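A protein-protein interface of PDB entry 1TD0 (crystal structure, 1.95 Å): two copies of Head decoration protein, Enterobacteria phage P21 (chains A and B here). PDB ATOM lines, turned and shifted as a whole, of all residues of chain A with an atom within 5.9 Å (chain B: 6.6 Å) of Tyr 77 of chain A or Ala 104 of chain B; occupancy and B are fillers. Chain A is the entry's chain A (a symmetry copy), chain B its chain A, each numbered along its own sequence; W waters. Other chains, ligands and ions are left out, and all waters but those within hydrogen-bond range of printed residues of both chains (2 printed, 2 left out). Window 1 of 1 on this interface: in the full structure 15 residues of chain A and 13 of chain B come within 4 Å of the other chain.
Tyr 77 of chain A touches one residue of chain B. Ala 104 of chain B touches two residues of chain A. Printed residues of chain A within 4 Å of Leu 108 of chain B: Lys 79 (3.9 Å). Of the printed residues of chain B, Gly 26 of chain A touches Asn 101 (3.0 Å). Printed residues of chain A within 4 Å of Ser 109 of chain B: Ala 24 (3.7 Å) and Lys 79 (2.8 Å). Printed residues of chain A within 4 Å of Ala 57 of chain B: Leu 42. Of the printed residues of chain B, Val 61 of chain A touches Gly 105 (3.6 Å). The nearest residue of chain B that does not touch Tyr 77 of chain A is Asn 101 of chain B (5.1 Å). The nearest printed residue of chain A that does not touch Asn 101 of chain B is Thr 25 of chain A (4.6 Å).
Ala 24 of chain A touches Ser 109 of chain B. Asn 101 of chain B touches Gly 26 of chain A. Leu 42 of chain A touches Ala 57 of chain B. Leu 42 of chain A touches Gly 58 of chain B (CD1 to CA, 3.6 Å). Asn 101 of chain B touches Leu 42 of chain A (CB to CD2, 3.9 Å). O of Ala 104 of chain B touches CD1 of Leu 42 of chain A, at 3.96 Å. ND2 of Asn 101 of chain B touches N of Leu 49 of chain A, at 3.5 Å. Gly 105 of chain B touches Val 61 of chain A (CA to CG1, 3.6 Å). Tyr 77 of chain A touches Ala 104 of chain B (OH to CB, 3.7 Å). Leu 108 of chain B touches Lys 79 of chain A (C to NZ, 3.9 Å).
No position is printed for both chains.
The side-chain hydroxyl (OG) of Ser 109 of chain B is in hydrogen-bond range of the side-chain amino group (NZ) of Lys 79 of chain A (2.8 Å).
N of Lys 79 of chain A is in hydrogen-bond range of O of His 22 of chain A. O of Leu 40 of chain A lies within hydrogen-bond range of N of Val 61 of chain A, 2.8 Å away. N of Gly 58 of chain B is in hydrogen-bond range of O of Asn 101 of chain B (2.9 Å). N of Leu 75 of chain A lies within hydrogen-bond range of O of Gly 26 of chain A, 2.9 Å away. The backbone NH (N) of Ala 24 of chain A lies within hydrogen-bond range of the backbone carbonyl oxygen (O) of Tyr 77 of chain A, 2.7 Å away. The backbone NH (N) of Gly 58 of chain B is in hydrogen-bond range of the backbone carbonyl oxygen (O) of Ala 102 of chain B (3.1 Å).
Hydrophobic or aromatic side chains of chain A that line the printed part of chain B: Ala 24, Leu 42, Leu 49, Val 61 and Tyr 77. Of the 13 printed residues of chain B, 7 touch a printed residue of chain A. Printed residues of chain B that touch a printed residue of chain A: Ala 57, Gly 58, Asn 101, Ala 104, Gly 105, Leu 108 and Ser 109. Hydrophobic or aromatic side chains of chain B within 4 Å of the printed part of chain A: Ala 57 and Ala 104. Among the printed residues, 11 pairs touch across the chains. Among the printed residues, no Asp or Glu carboxylate lies within 4 Å of a Lys or Arg side-chain nitrogen of the other chain.
Water W1 lies within hydrogen-bond range of the backbone carbonyl oxygen of Val 61 of chain A, the backbone NH of Gly 105 of chain B and the backbone carbonyl oxygen of Ser 106 of chain B. Water W2 lies within hydrogen-bond range of the side-chain hydroxyl (OH) of Tyr 77 of chain A (2.9 Å) and the backbone carbonyl oxygen (O) of Leu 108 of chain B (3.0 Å).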
ATOM      1  N   HIS A  22      -5.702  24.875  16.656  1.00  0.00           N
ATOM      2  CA  HIS A  22      -5.544  25.759  15.509  1.00  0.00           C
ATOM      3  C   HIS A  22      -6.727  26.705  15.539  1.00  0.00           C
ATOM      4  O   HIS A  22      -7.786  26.352  16.054  1.00  0.00           O
ATOM      5  CB  HIS A  22      -5.542  24.948  14.204  1.00  0.00           C
ATOM      6  CG  HIS A  22      -4.333  24.090  14.040  1.00  0.00           C
ATOM      7  ND1 HIS A  22      -4.406  22.753  13.718  1.00  0.00           N
ATOM      8  CD2 HIS A  22      -3.019  24.366  14.208  1.00  0.00           C
ATOM      9  CE1 HIS A  22      -3.191  22.239  13.705  1.00  0.00           C
ATOM     10  NE2 HIS A  22      -2.330  23.197  14.000  1.00  0.00           N
ATOM     11  N   THR A  23      -6.543  27.909  15.004  1.00  0.00           N
ATOM     12  CA  THR A  23      -7.609  28.906  14.976  1.00  0.00           C
ATOM     13  C   THR A  23      -8.049  29.250  13.554  1.00  0.00           C
ATOM     14  O   THR A  23      -7.377  28.918  12.577  1.00  0.00           O
ATOM     15  CB  THR A  23      -7.161  30.226  15.641  1.00  0.00           C
ATOM     16  OG1 THR A  23      -6.108  30.809  14.864  1.00  0.00           O
ATOM     17  CG2 THR A  23      -6.660  29.982  17.068  1.00  0.00           C
ATOM     18  N   ALA A  24      -9.191  29.918  13.454  1.00  0.00           N
ATOM     19  CA  ALA A  24      -9.741  30.344  12.179  1.00  0.00           C
ATOM     20  C   ALA A  24     -10.532  31.614  12.410  1.00  0.00           C
ATOM     21  O   ALA A  24     -10.818  31.985  13.553  1.00  0.00           O
ATOM     22  CB  ALA A  24     -10.655  29.270  11.601  1.00  0.00           C
ATOM     23  N   THR A  25     -10.879  32.282  11.318  1.00  0.00           N
ATOM     24  CA  THR A  25     -11.671  33.492  11.392  1.00  0.00           C
ATOM     25  C   THR A  25     -12.942  33.240  10.607  1.00  0.00           C
ATOM     26  O   THR A  25     -12.960  32.414   9.693  1.00  0.00           O
ATOM     27  CB  THR A  25     -10.929  34.694  10.774  1.00  0.00           C
ATOM     28  OG1 THR A  25     -10.552  34.384   9.425  1.00  0.00           O
ATOM     29  CG2 THR A  25      -9.692  35.030  11.588  1.00  0.00           C
ATOM     30  N   GLY A  26     -14.006  33.950  10.968  1.00  0.00           N
ATOM     31  CA  GLY A  26     -15.273  33.794  10.278  1.00  0.00           C
ATOM     32  C   GLY A  26     -16.242  34.919  10.611  1.00  0.00           C
ATOM     33  O   GLY A  26     -16.065  35.638  11.597  1.00  0.00           O
ATOM     34  N   LEU A  40     -19.404  27.999  19.780  1.00  0.00           N
ATOM     35  CA  LEU A  40     -20.056  28.659  18.657  1.00  0.00           C
ATOM     36  C   LEU A  40     -20.743  27.679  17.711  1.00  0.00           C
ATOM     37  O   LEU A  40     -20.269  26.566  17.515  1.00  0.00           O
ATOM     38  CB  LEU A  40     -19.016  29.460  17.866  1.00  0.00           C
ATOM     39  CG  LEU A  40     -18.190  30.444  18.692  1.00  0.00           C
ATOM     40  CD1 LEU A  40     -17.025  30.953  17.877  1.00  0.00           C
ATOM     41  CD2 LEU A  40     -19.090  31.594  19.144  1.00  0.00           C
ATOM     42  N   LEU A  42     -23.339  27.636  13.850  1.00  0.00           N
ATOM     43  CA  LEU A  42     -23.687  28.411  12.671  1.00  0.00           C
ATOM     44  C   LEU A  42     -25.166  28.778  12.694  1.00  0.00           C
ATOM     45  O   LEU A  42     -26.009  27.947  13.032  1.00  0.00           O
ATOM     46  CB  LEU A  42     -23.391  27.611  11.396  1.00  0.00           C
ATOM     47  CG  LEU A  42     -21.937  27.462  10.951  1.00  0.00           C
ATOM     48  CD1 LEU A  42     -21.869  26.458   9.810  1.00  0.00           C
ATOM     49  CD2 LEU A  42     -21.384  28.812  10.518  1.00  0.00           C
ATOM     50  N   LEU A  49     -21.543  32.996  12.375  1.00  0.00           N
ATOM     51  CA  LEU A  49     -21.275  32.266  13.606  1.00  0.00           C
ATOM     52  C   LEU A  49     -21.842  33.026  14.801  1.00  0.00           C
ATOM     53  O   LEU A  49     -21.617  34.235  14.944  1.00  0.00           O
ATOM     54  CB  LEU A  49     -19.774  32.073  13.791  1.00  0.00           C
ATOM     55  CG  LEU A  49     -19.098  31.091  12.828  1.00  0.00           C
ATOM     56  CD1 LEU A  49     -17.598  31.307  12.822  1.00  0.00           C
ATOM     57  CD2 LEU A  49     -19.441  29.666  13.257  1.00  0.00           C
ATOM     58  N   VAL A  61     -19.406  24.264  16.220  1.00  0.00           N
ATOM     59  CA  VAL A  61     -18.287  24.218  15.277  1.00  0.00           C
ATOM     60  C   VAL A  61     -17.027  24.984  15.685  1.00  0.00           C
ATOM     61  O   VAL A  61     -16.020  24.967  14.971  1.00  0.00           O
ATOM     62  CB  VAL A  61     -18.757  24.706  13.899  1.00  0.00           C
ATOM     63  CG1 VAL A  61     -19.933  23.878  13.451  1.00  0.00           C
ATOM     64  CG2 VAL A  61     -19.174  26.188  13.966  1.00  0.00           C
ATOM     65  N   GLY A  62     -17.068  25.650  16.838  1.00  0.00           N
ATOM     66  CA  GLY A  62     -15.895  26.372  17.284  1.00  0.00           C
ATOM     67  C   GLY A  62     -15.982  26.930  18.696  1.00  0.00           C
ATOM     68  O   GLY A  62     -17.035  26.901  19.324  1.00  0.00           O
ATOM     69  N   ILE A  63     -14.845  27.417  19.187  1.00  0.00           N
ATOM     70  CA  ILE A  63     -14.738  28.024  20.506  1.00  0.00           C
ATOM     71  C   ILE A  63     -14.109  29.412  20.326  1.00  0.00           C
ATOM     72  O   ILE A  63     -13.041  29.555  19.721  1.00  0.00           O
ATOM     73  CB  ILE A  63     -13.847  27.190  21.431  1.00  0.00           C
ATOM     74  CG1 ILE A  63     -14.505  25.824  21.696  1.00  0.00           C
ATOM     75  CG2 ILE A  63     -13.602  27.946  22.724  1.00  0.00           C
ATOM     76  CD1 ILE A  63     -13.645  24.873  22.488  1.00  0.00           C
ATOM     77  N   LEU A  64     -14.782  30.432  20.845  1.00  0.00           N
ATOM     78  CA  LEU A  64     -14.293  31.804  20.719  1.00  0.00           C
ATOM     79  C   LEU A  64     -12.899  31.931  21.328  1.00  0.00           C
ATOM     80  O   LEU A  64     -12.660  31.473  22.445  1.00  0.00           O
ATOM     81  CB  LEU A  64     -15.274  32.766  21.409  1.00  0.00           C
ATOM     82  CG  LEU A  64     -15.067  34.258  21.154  1.00  0.00           C
ATOM     83  CD1 LEU A  64     -15.148  34.544  19.657  1.00  0.00           C
ATOM     84  CD2 LEU A  64     -16.142  35.047  21.899  1.00  0.00           C
ATOM     85  N   VAL A  65     -11.970  32.531  20.591  1.00  0.00           N
ATOM     86  CA  VAL A  65     -10.610  32.690  21.106  1.00  0.00           C
ATOM     87  C   VAL A  65     -10.481  33.997  21.893  1.00  0.00           C
ATOM     88  O   VAL A  65      -9.900  34.016  22.985  1.00  0.00           O
ATOM     89  CB  VAL A  65      -9.568  32.681  19.962  1.00  0.00           C
ATOM     90  CG1 VAL A  65      -8.157  32.845  20.525  1.00  0.00           C
ATOM     91  CG2 VAL A  65      -9.670  31.380  19.180  1.00  0.00           C
ATOM     92  N   LEU A  75     -15.012  37.175  13.821  1.00  0.00           N
ATOM     93  CA  LEU A  75     -14.505  36.673  15.097  1.00  0.00           C
ATOM     94  C   LEU A  75     -13.434  35.623  14.838  1.00  0.00           C
ATOM     95  O   LEU A  75     -13.258  35.173  13.702  1.00  0.00           O
ATOM     96  CB  LEU A  75     -15.648  36.077  15.935  1.00  0.00           C
ATOM     97  CG  LEU A  75     -16.499  34.907  15.401  1.00  0.00           C
ATOM     98  CD1 LEU A  75     -15.645  33.660  15.216  1.00  0.00           C
ATOM     99  CD2 LEU A  75     -17.627  34.619  16.389  1.00  0.00           C
ATOM    100  N   THR A  76     -12.716  35.246  15.890  1.00  0.00           N
ATOM    101  CA  THR A  76     -11.656  34.251  15.798  1.00  0.00           C
ATOM    102  C   THR A  76     -12.011  33.061  16.683  1.00  0.00           C
ATOM    103  O   THR A  76     -12.411  33.219  17.833  1.00  0.00           O
ATOM    104  CB  THR A  76     -10.293  34.837  16.250  1.00  0.00           C
ATOM    105  OG1 THR A  76      -9.872  35.838  15.315  1.00  0.00           O
ATOM    106  CG2 THR A  76      -9.225  33.748  16.323  1.00  0.00           C
ATOM    107  N   TYR A  77     -11.868  31.862  16.140  1.00  0.00           N
ATOM    108  CA  TYR A  77     -12.202  30.678  16.904  1.00  0.00           C
ATOM    109  C   TYR A  77     -11.231  29.530  16.719  1.00  0.00           C
ATOM    110  O   TYR A  77     -10.552  29.427  15.695  1.00  0.00           O
ATOM    111  CB  TYR A  77     -13.618  30.208  16.547  1.00  0.00           C
ATOM    112  CG  TYR A  77     -13.813  29.762  15.102  1.00  0.00           C
ATOM    113  CD1 TYR A  77     -13.910  30.694  14.064  1.00  0.00           C
ATOM    114  CD2 TYR A  77     -13.959  28.406  14.785  1.00  0.00           C
ATOM    115  CE1 TYR A  77     -14.155  30.292  12.750  1.00  0.00           C
ATOM    116  CE2 TYR A  77     -14.210  27.988  13.477  1.00  0.00           C
ATOM    117  CZ  TYR A  77     -14.313  28.934  12.463  1.00  0.00           C
ATOM    118  OH  TYR A  77     -14.631  28.530  11.182  1.00  0.00           O
ATOM    119  N   TYR A  78     -11.142  28.681  17.736  1.00  0.00           N
ATOM    120  CA  TYR A  78     -10.303  27.502  17.649  1.00  0.00           C
ATOM    121  C   TYR A  78     -11.124  26.535  16.802  1.00  0.00           C
ATOM    122  O   TYR A  78     -12.342  26.429  16.981  1.00  0.00           O
ATOM    123  CB  TYR A  78     -10.071  26.875  19.029  1.00  0.00           C
ATOM    124  CG  TYR A  78      -9.321  27.740  20.010  1.00  0.00           C
ATOM    125  CD1 TYR A  78      -9.978  28.343  21.083  1.00  0.00           C
ATOM    126  CD2 TYR A  78      -7.949  27.922  19.896  1.00  0.00           C
ATOM    127  CE1 TYR A  78      -9.284  29.099  22.021  1.00  0.00           C
ATOM    128  CE2 TYR A  78      -7.240  28.683  20.829  1.00  0.00           C
ATOM    129  CZ  TYR A  78      -7.916  29.265  21.889  1.00  0.00           C
ATOM    130  OH  TYR A  78      -7.225  30.004  22.823  1.00  0.00           O
ATOM    131  N   LYS A  79     -10.471  25.846  15.868  1.00  0.00           N
ATOM    132  CA  LYS A  79     -11.173  24.888  15.019  1.00  0.00           C
ATOM    133  C   LYS A  79     -10.713  23.453  15.300  1.00  0.00           C
ATOM    134  O   LYS A  79     -11.247  22.510  14.734  1.00  0.00           O
ATOM    135  CB  LYS A  79     -10.954  25.216  13.536  1.00  0.00           C
ATOM    136  CG  LYS A  79      -9.501  25.160  13.078  1.00  0.00           C
ATOM    137  CD  LYS A  79      -9.426  25.103  11.539  1.00  0.00           C
ATOM    138  CE  LYS A  79      -7.998  24.904  11.031  1.00  0.00           C
ATOM    139  NZ  LYS A  79      -7.953  24.780   9.545  1.00  0.00           N
ATOM    140  N   ALA B  57     -23.650  27.812   4.958  1.00  0.00           N
ATOM    141  CA  ALA B  57     -22.360  27.938   5.601  1.00  0.00           C
ATOM    142  C   ALA B  57     -22.110  26.579   6.244  1.00  0.00           C
ATOM    143  O   ALA B  57     -23.049  25.938   6.698  1.00  0.00           O
ATOM    144  CB  ALA B  57     -22.418  29.023   6.677  1.00  0.00           C
ATOM    145  N   GLY B  58     -20.857  26.146   6.262  1.00  0.00           N
ATOM    146  CA  GLY B  58     -20.513  24.876   6.872  1.00  0.00           C
ATOM    147  C   GLY B  58     -20.860  23.620   6.086  1.00  0.00           C
ATOM    148  O   GLY B  58     -20.684  22.519   6.601  1.00  0.00           O
ATOM    149  N   SER B  59     -21.364  23.754   4.862  1.00  0.00           N
ATOM    150  CA  SER B  59     -21.691  22.556   4.083  1.00  0.00           C
ATOM    151  C   SER B  59     -20.554  22.154   3.148  1.00  0.00           C
ATOM    152  O   SER B  59     -20.644  21.136   2.451  1.00  0.00           O
ATOM    153  CB  SER B  59     -22.977  22.756   3.281  1.00  0.00           C
ATOM    154  OG  SER B  59     -22.785  23.681   2.224  1.00  0.00           O
ATOM    155  N   ALA B  60     -19.490  22.954   3.130  1.00  0.00           N
ATOM    156  CA  ALA B  60     -18.318  22.668   2.300  1.00  0.00           C
ATOM    157  C   ALA B  60     -17.392  21.752   3.093  1.00  0.00           C
ATOM    158  O   ALA B  60     -16.712  22.196   4.009  1.00  0.00           O
ATOM    159  CB  ALA B  60     -17.593  23.960   1.942  1.00  0.00           C
ATOM    160  N   ALA B 100     -17.365  32.982   3.937  1.00  0.00           N
ATOM    161  CA  ALA B 100     -16.395  33.078   5.022  1.00  0.00           C
ATOM    162  C   ALA B 100     -16.435  31.845   5.931  1.00  0.00           C
ATOM    163  O   ALA B 100     -15.402  31.366   6.409  1.00  0.00           O
ATOM    164  CB  ALA B 100     -16.672  34.320   5.841  1.00  0.00           C
ATOM    165  N   ASN B 101     -17.637  31.352   6.175  1.00  0.00           N
ATOM    166  CA  ASN B 101     -17.819  30.198   7.041  1.00  0.00           C
ATOM    167  C   ASN B 101     -18.171  28.937   6.264  1.00  0.00           C
ATOM    168  O   ASN B 101     -18.763  28.018   6.819  1.00  0.00           O
ATOM    169  CB  ASN B 101     -18.921  30.493   8.065  1.00  0.00           C
ATOM    170  CG  ASN B 101     -18.626  31.733   8.901  1.00  0.00           C
ATOM    171  OD1 ASN B 101     -17.477  32.150   9.025  1.00  0.00           O
ATOM    172  ND2 ASN B 101     -19.663  32.310   9.492  1.00  0.00           N
ATOM    173  N   ALA B 102     -17.801  28.886   4.985  1.00  0.00           N
ATOM    174  CA  ALA B 102     -18.120  27.723   4.167  1.00  0.00           C
ATOM    175  C   ALA B 102     -17.638  26.392   4.764  1.00  0.00           C
ATOM    176  O   ALA B 102     -18.338  25.381   4.670  1.00  0.00           O
ATOM    177  CB  ALA B 102     -17.547  27.898   2.770  1.00  0.00           C
ATOM    178  N   PHE B 103     -16.463  26.399   5.390  1.00  0.00           N
ATOM    179  CA  PHE B 103     -15.876  25.176   5.957  1.00  0.00           C
ATOM    180  C   PHE B 103     -16.042  24.995   7.467  1.00  0.00           C
ATOM    181  O   PHE B 103     -15.488  24.054   8.033  1.00  0.00           O
ATOM    182  CB  PHE B 103     -14.376  25.126   5.651  1.00  0.00           C
ATOM    183  CG  PHE B 103     -14.036  25.326   4.199  1.00  0.00           C
ATOM    184  CD1 PHE B 103     -13.375  26.483   3.784  1.00  0.00           C
ATOM    185  CD2 PHE B 103     -14.361  24.354   3.250  1.00  0.00           C
ATOM    186  CE1 PHE B 103     -13.040  26.676   2.446  1.00  0.00           C
ATOM    187  CE2 PHE B 103     -14.032  24.535   1.904  1.00  0.00           C
ATOM    188  CZ  PHE B 103     -13.369  25.701   1.501  1.00  0.00           C
ATOM    189  N   ALA B 104     -16.767  25.903   8.112  1.00  0.00           N
ATOM    190  CA  ALA B 104     -16.953  25.859   9.561  1.00  0.00           C
ATOM    191  C   ALA B 104     -17.556  24.531  10.019  1.00  0.00           C
ATOM    192  O   ALA B 104     -18.642  24.164   9.601  1.00  0.00           O
ATOM    193  CB  ALA B 104     -17.854  27.031  10.015  1.00  0.00           C
ATOM    194  N   GLY B 105     -16.850  23.832  10.892  1.00  0.00           N
ATOM    195  CA  GLY B 105     -17.339  22.553  11.380  1.00  0.00           C
ATOM    196  C   GLY B 105     -16.362  21.469  10.974  1.00  0.00           C
ATOM    197  O   GLY B 105     -16.254  20.436  11.629  1.00  0.00           O
ATOM    198  N   SER B 106     -15.628  21.713   9.891  1.00  0.00           N
ATOM    199  CA  SER B 106     -14.653  20.736   9.417  1.00  0.00           C
ATOM    200  C   SER B 106     -13.275  21.160   9.884  1.00  0.00           C
ATOM    201  O   SER B 106     -13.129  22.121  10.663  1.00  0.00           O
ATOM    202  CB  SER B 106     -14.690  20.665   7.893  1.00  0.00           C
ATOM    203  OG  SER B 106     -14.005  21.765   7.348  1.00  0.00           O
ATOM    204  N   LEU B 108     -11.087  22.246   7.890  1.00  0.00           N
ATOM    205  CA  LEU B 108     -10.666  23.229   6.890  1.00  0.00           C
ATOM    206  C   LEU B 108     -11.079  24.659   7.240  1.00  0.00           C
ATOM    207  O   LEU B 108     -12.098  24.888   7.865  1.00  0.00           O
ATOM    208  CB  LEU B 108     -11.301  22.891   5.534  1.00  0.00           C
ATOM    209  CG  LEU B 108     -10.926  21.582   4.826  1.00  0.00           C
ATOM    210  CD1 LEU B 108     -11.863  21.352   3.673  1.00  0.00           C
ATOM    211  CD2 LEU B 108      -9.493  21.648   4.360  1.00  0.00           C
ATOM    212  N   SER B 109     -10.286  25.612   6.788  1.00  0.00           N
ATOM    213  CA  SER B 109     -10.596  27.016   6.996  1.00  0.00           C
ATOM    214  C   SER B 109      -9.870  27.768   5.898  1.00  0.00           C
ATOM    215  O   SER B 109      -9.067  27.179   5.161  1.00  0.00           O
ATOM    216  CB  SER B 109     -10.115  27.483   8.362  1.00  0.00           C
ATOM    217  OG  SER B 109      -8.750  27.261   8.516  1.00  0.00           O
HETATM  218  O   HOH W   1     -14.526  24.236  12.885  1.00  0.00           O
HETATM  219  O   HOH W   2     -13.510  27.336   8.736  1.00  0.00           O
